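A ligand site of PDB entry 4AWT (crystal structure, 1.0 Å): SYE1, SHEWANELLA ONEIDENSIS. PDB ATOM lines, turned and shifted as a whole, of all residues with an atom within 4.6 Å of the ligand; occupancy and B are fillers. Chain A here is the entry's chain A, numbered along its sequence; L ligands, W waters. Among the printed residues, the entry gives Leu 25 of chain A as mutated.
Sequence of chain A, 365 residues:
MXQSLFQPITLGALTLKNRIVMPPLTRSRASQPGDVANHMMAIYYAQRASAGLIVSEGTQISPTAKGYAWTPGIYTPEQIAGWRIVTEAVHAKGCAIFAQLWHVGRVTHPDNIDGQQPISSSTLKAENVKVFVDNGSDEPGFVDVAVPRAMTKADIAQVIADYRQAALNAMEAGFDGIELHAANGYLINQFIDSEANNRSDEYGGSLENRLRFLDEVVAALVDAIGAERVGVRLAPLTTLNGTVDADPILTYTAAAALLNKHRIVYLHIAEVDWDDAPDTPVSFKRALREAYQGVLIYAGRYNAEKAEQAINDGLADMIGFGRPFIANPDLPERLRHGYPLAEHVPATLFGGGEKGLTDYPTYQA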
ATOM      1  N   PRO A  23       4.065  25.229 -15.226  1.00  0.00           N
ATOM      2  CA  PRO A  23       4.659  26.568 -15.247  1.00  0.00           C
ATOM      3  C   PRO A  23       4.912  26.947 -16.699  1.00  0.00           C
ATOM      4  O   PRO A  23       4.795  26.129 -17.611  1.00  0.00           O
ATOM      5  CB  PRO A  23       5.966  26.339 -14.485  1.00  0.00           C
ATOM      6  CG  PRO A  23       6.392  24.953 -14.917  1.00  0.00           C
ATOM      7  CD  PRO A  23       5.079  24.162 -15.032  1.00  0.00           C
ATOM      8  N   PRO A  24       5.302  28.212 -16.909  1.00  0.00           N
ATOM      9  CA  PRO A  24       5.578  28.707 -18.259  1.00  0.00           C
ATOM     10  C   PRO A  24       6.688  27.916 -18.912  1.00  0.00           C
ATOM     11  O   PRO A  24       7.772  27.744 -18.357  1.00  0.00           O
ATOM     12  CB  PRO A  24       6.018  30.146 -18.028  1.00  0.00           C
ATOM     13  CG  PRO A  24       5.263  30.539 -16.834  1.00  0.00           C
ATOM     14  CD  PRO A  24       5.403  29.311 -15.944  1.00  0.00           C
ATOM     15  N   LEU A  25       6.450  27.475 -20.172  1.00  0.00           N
ATOM     16  CA  LEU A  25       7.437  26.708 -20.928  1.00  0.00           C
ATOM     17  C   LEU A  25       7.417  27.178 -22.373  1.00  0.00           C
ATOM     18  O   LEU A  25       6.595  26.726 -23.184  1.00  0.00           O
ATOM     19  CB  LEU A  25       7.151  25.198 -20.857  1.00  0.00           C
ATOM     20  CG  LEU A  25       7.168  24.608 -19.442  1.00  0.00           C
ATOM     21  CD1 LEU A  25       6.331  23.328 -19.412  1.00  0.00           C
ATOM     22  CD2 LEU A  25       8.612  24.352 -18.972  1.00  0.00           C
ATOM     23  N   THR A  26       8.320  28.047 -22.728  1.00  0.00           N
ATOM     24  CA  THR A  26       8.530  28.483 -24.124  1.00  0.00           C
ATOM     25  C   THR A  26       8.767  27.271 -24.998  1.00  0.00           C
ATOM     26  O   THR A  26       9.695  26.497 -24.763  1.00  0.00           O
ATOM     27  CB  THR A  26       9.755  29.414 -24.177  1.00  0.00           C
ATOM     28  OG1 THR A  26       9.457  30.670 -23.566  1.00  0.00           O
ATOM     29  CG2 THR A  26      10.225  29.698 -25.583  1.00  0.00           C
ATOM     30  N   GLU A  57       3.460  29.712 -21.588  1.00  0.00           N
ATOM     31  CA  GLU A  57       4.757  30.186 -21.982  1.00  0.00           C
ATOM     32  C   GLU A  57       4.771  31.715 -22.044  1.00  0.00           C
ATOM     33  O   GLU A  57       3.747  32.362 -22.317  1.00  0.00           O
ATOM     34  CB  GLU A  57       5.154  29.610 -23.344  1.00  0.00           C
ATOM     35  CG  GLU A  57       4.230  30.005 -24.518  1.00  0.00           C
ATOM     36  CD  GLU A  57       4.241  28.883 -25.547  1.00  0.00           C
ATOM     37  OE1 GLU A  57       5.264  28.684 -26.244  1.00  0.00           O
ATOM     38  OE2 GLU A  57       3.202  28.189 -25.661  1.00  0.00           O
ATOM     39  N   GLY A  58       5.950  32.291 -21.873  1.00  0.00           N
ATOM     40  CA  GLY A  58       6.050  33.741 -21.985  1.00  0.00           C
ATOM     41  C   GLY A  58       5.494  34.197 -23.326  1.00  0.00           C
ATOM     42  O   GLY A  58       5.758  33.640 -24.384  1.00  0.00           O
ATOM     43  N   GLN A 100       1.477  34.398 -19.253  1.00  0.00           N
ATOM     44  CA  GLN A 100       2.701  34.993 -18.733  1.00  0.00           C
ATOM     45  C   GLN A 100       3.143  36.144 -19.620  1.00  0.00           C
ATOM     46  O   GLN A 100       3.644  35.954 -20.715  1.00  0.00           O
ATOM     47  CB  GLN A 100       3.836  33.988 -18.590  1.00  0.00           C
ATOM     48  CG  GLN A 100       4.991  34.675 -17.872  1.00  0.00           C
ATOM     49  CD  GLN A 100       6.247  33.875 -17.833  1.00  0.00           C
ATOM     50  OE1 GLN A 100       6.838  33.539 -18.875  1.00  0.00           O
ATOM     51  NE2 GLN A 100       6.740  33.608 -16.625  1.00  0.00           N
ATOM     52  N   TRP A 102       5.430  38.903 -21.015  1.00  0.00           N
ATOM     53  CA  TRP A 102       6.884  38.851 -21.118  1.00  0.00           C
ATOM     54  C   TRP A 102       7.461  40.128 -21.745  1.00  0.00           C
ATOM     55  O   TRP A 102       7.034  40.545 -22.824  1.00  0.00           O
ATOM     56  CB  TRP A 102       7.306  37.669 -21.990  1.00  0.00           C
ATOM     57  CG  TRP A 102       8.648  37.086 -21.709  1.00  0.00           C
ATOM     58  CD1 TRP A 102       9.556  37.368 -20.724  1.00  0.00           C
ATOM     59  CD2 TRP A 102       9.200  36.007 -22.463  1.00  0.00           C
ATOM     60  NE1 TRP A 102      10.627  36.507 -20.817  1.00  0.00           N
ATOM     61  CE2 TRP A 102      10.421  35.653 -21.859  1.00  0.00           C
ATOM     62  CE3 TRP A 102       8.751  35.277 -23.567  1.00  0.00           C
ATOM     63  CZ2 TRP A 102      11.185  34.595 -22.338  1.00  0.00           C
ATOM     64  CZ3 TRP A 102       9.520  34.226 -24.015  1.00  0.00           C
ATOM     65  CH2 TRP A 102      10.685  33.904 -23.424  1.00  0.00           C
ATOM     66  N   HIS A 181       6.133  38.140 -15.748  1.00  0.00           N
ATOM     67  CA  HIS A 181       7.458  37.523 -15.702  1.00  0.00           C
ATOM     68  C   HIS A 181       8.442  38.590 -15.203  1.00  0.00           C
ATOM     69  O   HIS A 181       8.883  39.438 -15.981  1.00  0.00           O
ATOM     70  CB  HIS A 181       7.890  37.007 -17.060  1.00  0.00           C
ATOM     71  CG  HIS A 181       9.043  36.055 -16.994  1.00  0.00           C
ATOM     72  ND1 HIS A 181       9.799  35.912 -15.889  1.00  0.00           N
ATOM     73  CD2 HIS A 181       9.443  35.164 -17.949  1.00  0.00           C
ATOM     74  CE1 HIS A 181      10.675  34.966 -16.173  1.00  0.00           C
ATOM     75  NE2 HIS A 181      10.488  34.483 -17.382  1.00  0.00           N
ATOM     76  N   ASN A 184      14.077  35.330 -14.023  1.00  0.00           N
ATOM     77  CA  ASN A 184      15.019  34.687 -14.918  1.00  0.00           C
ATOM     78  C   ASN A 184      15.749  35.707 -15.810  1.00  0.00           C
ATOM     79  O   ASN A 184      16.057  35.411 -16.967  1.00  0.00           O
ATOM     80  CB  ASN A 184      14.338  33.582 -15.711  1.00  0.00           C
ATOM     81  CG  ASN A 184      13.836  32.511 -14.766  1.00  0.00           C
ATOM     82  OD1 ASN A 184      14.133  32.505 -13.592  1.00  0.00           O
ATOM     83  ND2 ASN A 184      13.068  31.598 -15.292  1.00  0.00           N
ATOM     84  N   ARG A 233       6.051  36.360 -11.102  1.00  0.00           N
ATOM     85  CA  ARG A 233       7.144  35.401 -10.993  1.00  0.00           C
ATOM     86  C   ARG A 233       8.438  36.146 -10.689  1.00  0.00           C
ATOM     87  O   ARG A 233       8.778  37.121 -11.349  1.00  0.00           O
ATOM     88  CB  ARG A 233       7.289  34.591 -12.280  1.00  0.00           C
ATOM     89  CG  ARG A 233       8.005  33.263 -12.005  1.00  0.00           C
ATOM     90  CD  ARG A 233       8.011  32.322 -13.183  1.00  0.00           C
ATOM     91  NE  ARG A 233       8.224  30.961 -12.702  1.00  0.00           N
ATOM     92  CZ  ARG A 233       8.688  29.922 -13.396  1.00  0.00           C
ATOM     93  NH1 ARG A 233       9.219  30.061 -14.575  1.00  0.00           N
ATOM     94  NH2 ARG A 233       8.659  28.721 -12.825  1.00  0.00           N
ATOM     95  N   ALA A 270      10.708  30.968  -9.141  1.00  0.00           N
ATOM     96  CA  ALA A 270      11.453  30.109 -10.040  1.00  0.00           C
ATOM     97  C   ALA A 270      12.758  29.745  -9.328  1.00  0.00           C
ATOM     98  O   ALA A 270      13.707  30.525  -9.266  1.00  0.00           O
ATOM     99  CB  ALA A 270      11.723  30.813 -11.339  1.00  0.00           C
ATOM    100  N   VAL A 272      14.817  27.046  -9.705  1.00  0.00           N
ATOM    101  CA  VAL A 272      15.859  26.497 -10.568  1.00  0.00           C
ATOM    102  C   VAL A 272      15.651  27.056 -11.947  1.00  0.00           C
ATOM    103  O   VAL A 272      14.485  27.181 -12.372  1.00  0.00           O
ATOM    104  CB  VAL A 272      15.783  24.967 -10.611  1.00  0.00           C
ATOM    105  CG1 VAL A 272      16.802  24.389 -11.605  1.00  0.00           C
ATOM    106  CG2 VAL A 272      15.957  24.347  -9.236  1.00  0.00           C
ATOM    107  N   ASP A 273      16.727  27.377 -12.654  1.00  0.00           N
ATOM    108  CA  ASP A 273      16.593  27.667 -14.061  1.00  0.00           C
ATOM    109  C   ASP A 273      17.642  26.824 -14.775  1.00  0.00           C
ATOM    110  O   ASP A 273      18.857  26.951 -14.576  1.00  0.00           O
ATOM    111  CB  ASP A 273      16.752  29.155 -14.347  1.00  0.00           C
ATOM    112  CG  ASP A 273      16.146  29.602 -15.649  1.00  0.00           C
ATOM    113  OD1 ASP A 273      15.069  29.108 -16.014  1.00  0.00           O
ATOM    114  OD2 ASP A 273      16.750  30.518 -16.273  1.00  0.00           O
ATOM    115  N   TRP A 274      17.134  25.846 -15.511  1.00  0.00           N
ATOM    116  CA  TRP A 274      17.943  24.829 -16.193  1.00  0.00           C
ATOM    117  C   TRP A 274      18.762  24.059 -15.150  1.00  0.00           C
ATOM    118  O   TRP A 274      18.178  23.292 -14.374  1.00  0.00           O
ATOM    119  CB  TRP A 274      18.727  25.406 -17.329  1.00  0.00           C
ATOM    120  CG  TRP A 274      17.817  25.898 -18.393  1.00  0.00           C
ATOM    121  CD1 TRP A 274      17.478  27.174 -18.656  1.00  0.00           C
ATOM    122  CD2 TRP A 274      17.101  25.092 -19.322  1.00  0.00           C
ATOM    123  NE1 TRP A 274      16.604  27.228 -19.694  1.00  0.00           N
ATOM    124  CE2 TRP A 274      16.361  25.967 -20.120  1.00  0.00           C
ATOM    125  CE3 TRP A 274      16.993  23.732 -19.568  1.00  0.00           C
ATOM    126  CZ2 TRP A 274      15.534  25.533 -21.161  1.00  0.00           C
ATOM    127  CZ3 TRP A 274      16.164  23.325 -20.625  1.00  0.00           C
ATOM    128  CH2 TRP A 274      15.462  24.239 -21.380  1.00  0.00           C
ATOM    129  N   ALA A 299       8.650  26.393  -8.388  1.00  0.00           N
ATOM    130  CA  ALA A 299       8.998  25.433  -9.428  1.00  0.00           C
ATOM    131  C   ALA A 299      10.512  25.331  -9.505  1.00  0.00           C
ATOM    132  O   ALA A 299      11.222  26.330  -9.321  1.00  0.00           O
ATOM    133  CB  ALA A 299       8.490  25.858 -10.798  1.00  0.00           C
ATOM    134  N   GLY A 300      10.992  24.129  -9.798  1.00  0.00           N
ATOM    135  CA  GLY A 300      12.410  23.889 -10.049  1.00  0.00           C
ATOM    136  C   GLY A 300      12.826  22.567  -9.394  1.00  0.00           C
ATOM    137  O   GLY A 300      12.989  22.493  -8.195  1.00  0.00           O
ATOM    138  N   ARG A 301      12.989  21.557 -10.261  1.00  0.00           N
ATOM    139  CA  ARG A 301      13.489  20.248  -9.834  1.00  0.00           C
ATOM    140  C   ARG A 301      12.602  19.590  -8.766  1.00  0.00           C
ATOM    141  O   ARG A 301      13.099  18.777  -7.983  1.00  0.00           O
ATOM    142  CB  ARG A 301      14.956  20.219  -9.446  1.00  0.00           C
ATOM    143  CG  ARG A 301      15.877  20.545 -10.600  1.00  0.00           C
ATOM    144  CD  ARG A 301      15.766  19.605 -11.764  1.00  0.00           C
ATOM    145  NE  ARG A 301      16.915  19.729 -12.672  1.00  0.00           N
ATOM    146  CZ  ARG A 301      16.961  19.236 -13.906  1.00  0.00           C
ATOM    147  NH1 ARG A 301      15.938  18.625 -14.445  1.00  0.00           N
ATOM    148  NH2 ARG A 301      18.087  19.403 -14.595  1.00  0.00           N
ATOM    149  N   GLY A 320       5.005  23.842  -9.277  1.00  0.00           N
ATOM    150  CA  GLY A 320       5.104  23.674 -10.685  1.00  0.00           C
ATOM    151  C   GLY A 320       6.141  22.633 -11.067  1.00  0.00           C
ATOM    152  O   GLY A 320       7.173  22.506 -10.425  1.00  0.00           O
ATOM    153  N   PHE A 321       5.836  21.918 -12.156  1.00  0.00           N
ATOM    154  CA  PHE A 321       6.716  20.901 -12.736  1.00  0.00           C
ATOM    155  C   PHE A 321       6.897  21.273 -14.195  1.00  0.00           C
ATOM    156  O   PHE A 321       5.906  21.246 -14.952  1.00  0.00           O
ATOM    157  CB  PHE A 321       6.104  19.500 -12.636  1.00  0.00           C
ATOM    158  CG  PHE A 321       5.791  19.084 -11.226  1.00  0.00           C
ATOM    159  CD1 PHE A 321       4.627  19.468 -10.610  1.00  0.00           C
ATOM    160  CD2 PHE A 321       6.658  18.297 -10.501  1.00  0.00           C
ATOM    161  CE1 PHE A 321       4.306  19.093  -9.329  1.00  0.00           C
ATOM    162  CE2 PHE A 321       6.335  17.903  -9.216  1.00  0.00           C
ATOM    163  CZ  PHE A 321       5.144  18.276  -8.652  1.00  0.00           C
ATOM    164  N   GLY A 322       8.096  21.693 -14.586  1.00  0.00           N
ATOM    165  CA  GLY A 322       8.318  22.192 -15.932  1.00  0.00           C
ATOM    166  C   GLY A 322       8.656  21.077 -16.890  1.00  0.00           C
ATOM    167  O   GLY A 322       7.834  20.569 -17.632  1.00  0.00           O
ATOM    168  N   ARG A 323       9.930  20.661 -16.837  1.00  0.00           N
ATOM    169  CA  ARG A 323      10.403  19.583 -17.734  1.00  0.00           C
ATOM    170  C   ARG A 323       9.529  18.366 -17.663  1.00  0.00           C
ATOM    171  O   ARG A 323       9.206  17.802 -18.729  1.00  0.00           O
ATOM    172  CB  ARG A 323      11.901  19.357 -17.515  1.00  0.00           C
ATOM    173  CG  ARG A 323      12.680  20.499 -18.137  1.00  0.00           C
ATOM    174  CD  ARG A 323      14.120  20.638 -17.656  1.00  0.00           C
ATOM    175  NE  ARG A 323      14.176  21.209 -16.330  1.00  0.00           N
ATOM    176  CZ  ARG A 323      15.294  21.612 -15.774  1.00  0.00           C
ATOM    177  NH1 ARG A 323      16.441  21.464 -16.442  1.00  0.00           N
ATOM    178  NH2 ARG A 323      15.284  22.180 -14.562  1.00  0.00           N
ATOM    179  N   PRO A 324       9.073  17.892 -16.488  1.00  0.00           N
ATOM    180  CA  PRO A 324       8.224  16.702 -16.516  1.00  0.00           C
ATOM    181  C   PRO A 324       6.901  16.897 -17.252  1.00  0.00           C
ATOM    182  O   PRO A 324       6.379  15.960 -17.819  1.00  0.00           O
ATOM    183  CB  PRO A 324       7.980  16.403 -15.029  1.00  0.00           C
ATOM    184  CG  PRO A 324       9.257  16.948 -14.355  1.00  0.00           C
ATOM    185  CD  PRO A 324       9.523  18.242 -15.123  1.00  0.00           C
ATOM    186  N   ILE A 326       6.505  18.600 -19.971  1.00  0.00           N
ATOM    187  CA  ILE A 326       6.686  18.534 -21.408  1.00  0.00           C
ATOM    188  C   ILE A 326       6.431  17.115 -21.897  1.00  0.00           C
ATOM    189  O   ILE A 326       5.739  16.932 -22.887  1.00  0.00           O
ATOM    190  CB  ILE A 326       8.095  19.018 -21.736  1.00  0.00           C
ATOM    191  CG1 ILE A 326       8.173  20.511 -21.412  1.00  0.00           C
ATOM    192  CG2 ILE A 326       8.538  18.681 -23.159  1.00  0.00           C
ATOM    193  CD1 ILE A 326       9.591  21.030 -21.591  1.00  0.00           C
ATOM    194  N   LEU A 349      12.410  20.796 -27.923  1.00  0.00           N
ATOM    195  CA  LEU A 349      11.865  21.800 -27.008  1.00  0.00           C
ATOM    196  C   LEU A 349      11.369  23.028 -27.775  1.00  0.00           C
ATOM    197  O   LEU A 349      10.330  23.567 -27.425  1.00  0.00           O
ATOM    198  CB  LEU A 349      12.850  22.188 -25.947  1.00  0.00           C
ATOM    199  CG  LEU A 349      13.081  21.107 -24.894  1.00  0.00           C
ATOM    200  CD1 LEU A 349      14.177  21.518 -23.963  1.00  0.00           C
ATOM    201  CD2 LEU A 349      11.822  20.830 -24.092  1.00  0.00           C
ATOM    202  N   PHE A 350      12.158  23.499 -28.743  1.00  0.00           N
ATOM    203  CA  PHE A 350      11.969  24.786 -29.358  1.00  0.00           C
ATOM    204  C   PHE A 350      11.838  24.651 -30.861  1.00  0.00           C
ATOM    205  O   PHE A 350      12.713  24.060 -31.516  1.00  0.00           O
ATOM    206  CB  PHE A 350      13.145  25.739 -29.071  1.00  0.00           C
ATOM    207  CG  PHE A 350      13.455  25.863 -27.611  1.00  0.00           C
ATOM    208  CD1 PHE A 350      12.543  26.397 -26.731  1.00  0.00           C
ATOM    209  CD2 PHE A 350      14.651  25.430 -27.127  1.00  0.00           C
ATOM    210  CE1 PHE A 350      12.828  26.533 -25.398  1.00  0.00           C
ATOM    211  CE2 PHE A 350      14.948  25.532 -25.804  1.00  0.00           C
ATOM    212  CZ  PHE A 350      14.037  26.081 -24.951  1.00  0.00           C
HETATM  213  N1  LIG L   1      10.088  30.108 -17.391  1.00  0.00           N
HETATM  214  C1  LIG L   1       9.344  31.193 -17.567  1.00  0.00           C
HETATM  215  O1  LIG L   1       9.044  31.964 -16.615  1.00  0.00           O
HETATM  216  N2  LIG L   1       8.887  31.515 -18.839  1.00  0.00           N
HETATM  217  C2  LIG L   1       9.153  30.748 -19.957  1.00  0.00           C
HETATM  218  O2  LIG L   1       8.612  31.056 -21.046  1.00  0.00           O
HETATM  219  C3  LIG L   1      10.019  29.678 -19.766  1.00  0.00           C
HETATM  220  N3  LIG L   1      10.437  28.901 -20.845  1.00  0.00           N
HETATM  221  C4  LIG L   1      10.939  27.599 -20.558  1.00  0.00           C
HETATM  222  C5  LIG L   1      11.115  26.696 -21.579  1.00  0.00           C
HETATM  223  C6  LIG L   1      11.581  25.385 -21.340  1.00  0.00           C
HETATM  224  C7  LIG L   1      11.625  24.406 -22.495  1.00  0.00           C
HETATM  225  C8  LIG L   1      11.934  25.049 -20.069  1.00  0.00           C
HETATM  226  C9  LIG L   1      12.416  23.651 -19.717  1.00  0.00           C
HETATM  227  C10 LIG L   1      11.776  25.969 -19.015  1.00  0.00           C
HETATM  228  C11 LIG L   1      11.272  27.252 -19.252  1.00  0.00           C
HETATM  229  N4  LIG L   1      11.051  28.159 -18.186  1.00  0.00           N
HETATM  230  C12 LIG L   1      10.375  29.335 -18.438  1.00  0.00           C
HETATM  231  C13 LIG L   1      11.349  27.747 -16.814  1.00  0.00           C
HETATM  232  C14 LIG L   1      10.308  26.789 -16.221  1.00  0.00           C
HETATM  233  O3  LIG L   1       9.077  27.465 -15.996  1.00  0.00           O
HETATM  234  C15 LIG L   1      10.727  26.216 -14.889  1.00  0.00           C
HETATM  235  O4  LIG L   1      10.807  27.204 -13.879  1.00  0.00           O
HETATM  236  C16 LIG L   1      12.056  25.427 -14.913  1.00  0.00           C
HETATM  237  O5  LIG L   1      12.128  24.560 -16.026  1.00  0.00           O
HETATM  238  C17 LIG L   1      12.328  24.714 -13.603  1.00  0.00           C
HETATM  239  O6  LIG L   1      11.320  23.719 -13.328  1.00  0.00           O
HETATM  240  P1  LIG L   1      11.615  22.167 -13.670  1.00  0.00           P
HETATM  241  O7  LIG L   1      11.692  22.061 -15.172  1.00  0.00           O
HETATM  242  O8  LIG L   1      12.928  21.801 -13.009  1.00  0.00           O
HETATM  243  O9  LIG L   1      10.423  21.463 -13.088  1.00  0.00           O
HETATM  244  O   HOH W   1      14.715  25.076 -16.904  1.00  0.00           O
HETATM  245  O   HOH W   2      13.097  28.756 -14.159  1.00  0.00           O
HETATM  246  O   HOH W   3      13.303  19.054 -13.544  1.00  0.00           O
HETATM  247  O   HOH W   4       9.756  21.692 -10.490  1.00  0.00           O
HETATM  248  O   HOH W   5      10.766  18.840 -12.080  1.00  0.00           O
HETATM  249  O   HOH W   6      12.158  32.152 -18.082  1.00  0.00           O
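ND2 of Asn 184 sits at hydrogen-bond distance from OD1 of Asp 273 (3.3 Å).
The side-chain amide oxygen (OE1) of Gln 100 lies close to the backbone NH (N) of Gly 58 (3.4 Å).
The guanidinium group of Arg 323 lies within hydrogen-bond range of the backbone carbonyl oxygen of Trp 274, 3.1 Å away.
The backbone NH (N) of Thr 26 is in hydrogen-bond range of a nitrogen (N3) of the ligand, 3.0 Å away.
N of Arg 301 is in hydrogen-bond range of O8 of the ligand (2.8 Å).
The guanidinium group (NH2) of Arg 323 is in salt-bridge range of an oxygen (O8) of the ligand (2.8 Å).
NE2 of His 181 sits at hydrogen-bond distance from O1 of the ligand (3.0 Å).
N of Arg 323 sits at hydrogen-bond distance from O7 of the ligand (2.8 Å).
O1 of the ligand lies within hydrogen-bond range of NE2 of Gln 100, 2.8 Å away.
O9 of the ligand sits at hydrogen-bond distance from N of Gly 322, 2.8 Å away.
N of Gly 58 is in hydrogen-bond range of O2 of the ligand.
An oxygen (O1) of the ligand lies within hydrogen-bond range of the guanidinium group of Arg 233, at 2.8 Å.
An oxygen (O2) of the ligand is in hydrogen-bond range of the side-chain hydroxyl (OG1) of Thr 26.
O3 of the ligand is in hydrogen-bond range of O of Pro 24 (2.7 Å).
Pro 23 touches the ligand.
CD2 of Leu 25 touches C10 of the ligand, 3.6 Å away.
Asn 184 touches the ligand.
O of Val 272 touches C17 of the ligand, 3.5 Å away.
Trp 274 touches the ligand (CH2 to C9, 3.5 Å).
Gly 300 touches the ligand.
C of Phe 321 touches O9 of the ligand (3.7 Å).
CD of Pro 324 touches O9 of the ligand, 3.9 Å away.
Leu 349 touches the ligand.
CE1 of Phe 350 touches C7 of the ligand (3.8 Å).
Hydrophobic or aromatic side chains that line the ligand: Pro 23, Pro 24, Leu 25, His 181, Trp 274, Pro 324, Leu 349 and Phe 350.
The nearest printed residue that does not touch the ligand is Glu 57 (4.02 Å).
Water W4 lies within hydrogen-bond range of O9 of the ligand (2.7 Å), O of Gly 320 (2.7 Å), N of Gly 300 (2.8 Å) and N of Arg 301 (3.2 Å).
Water W1 lies within hydrogen-bond range of O5 of the ligand (2.8 Å) and N of Trp 274 (2.9 Å).
Water W2 lies within hydrogen-bond range of the side-chain carboxylate of Asp 273 (2.7 Å), the backbone carbonyl oxygen of Val 272 (2.8 Å), an oxygen (O4) of the ligand (2.8 Å) and the side-chain amide nitrogen of Asn 184 (3.1 Å).
Water W3 lies within hydrogen-bond range of the guanidinium group (NH1) of Arg 301 (2.8 Å) and an oxygen (O8) of the ligand (2.8 Å).
Water W6 lies within hydrogen-bond range of NE2 of His 181, ND2 of Asn 184 and N1 of the ligand.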
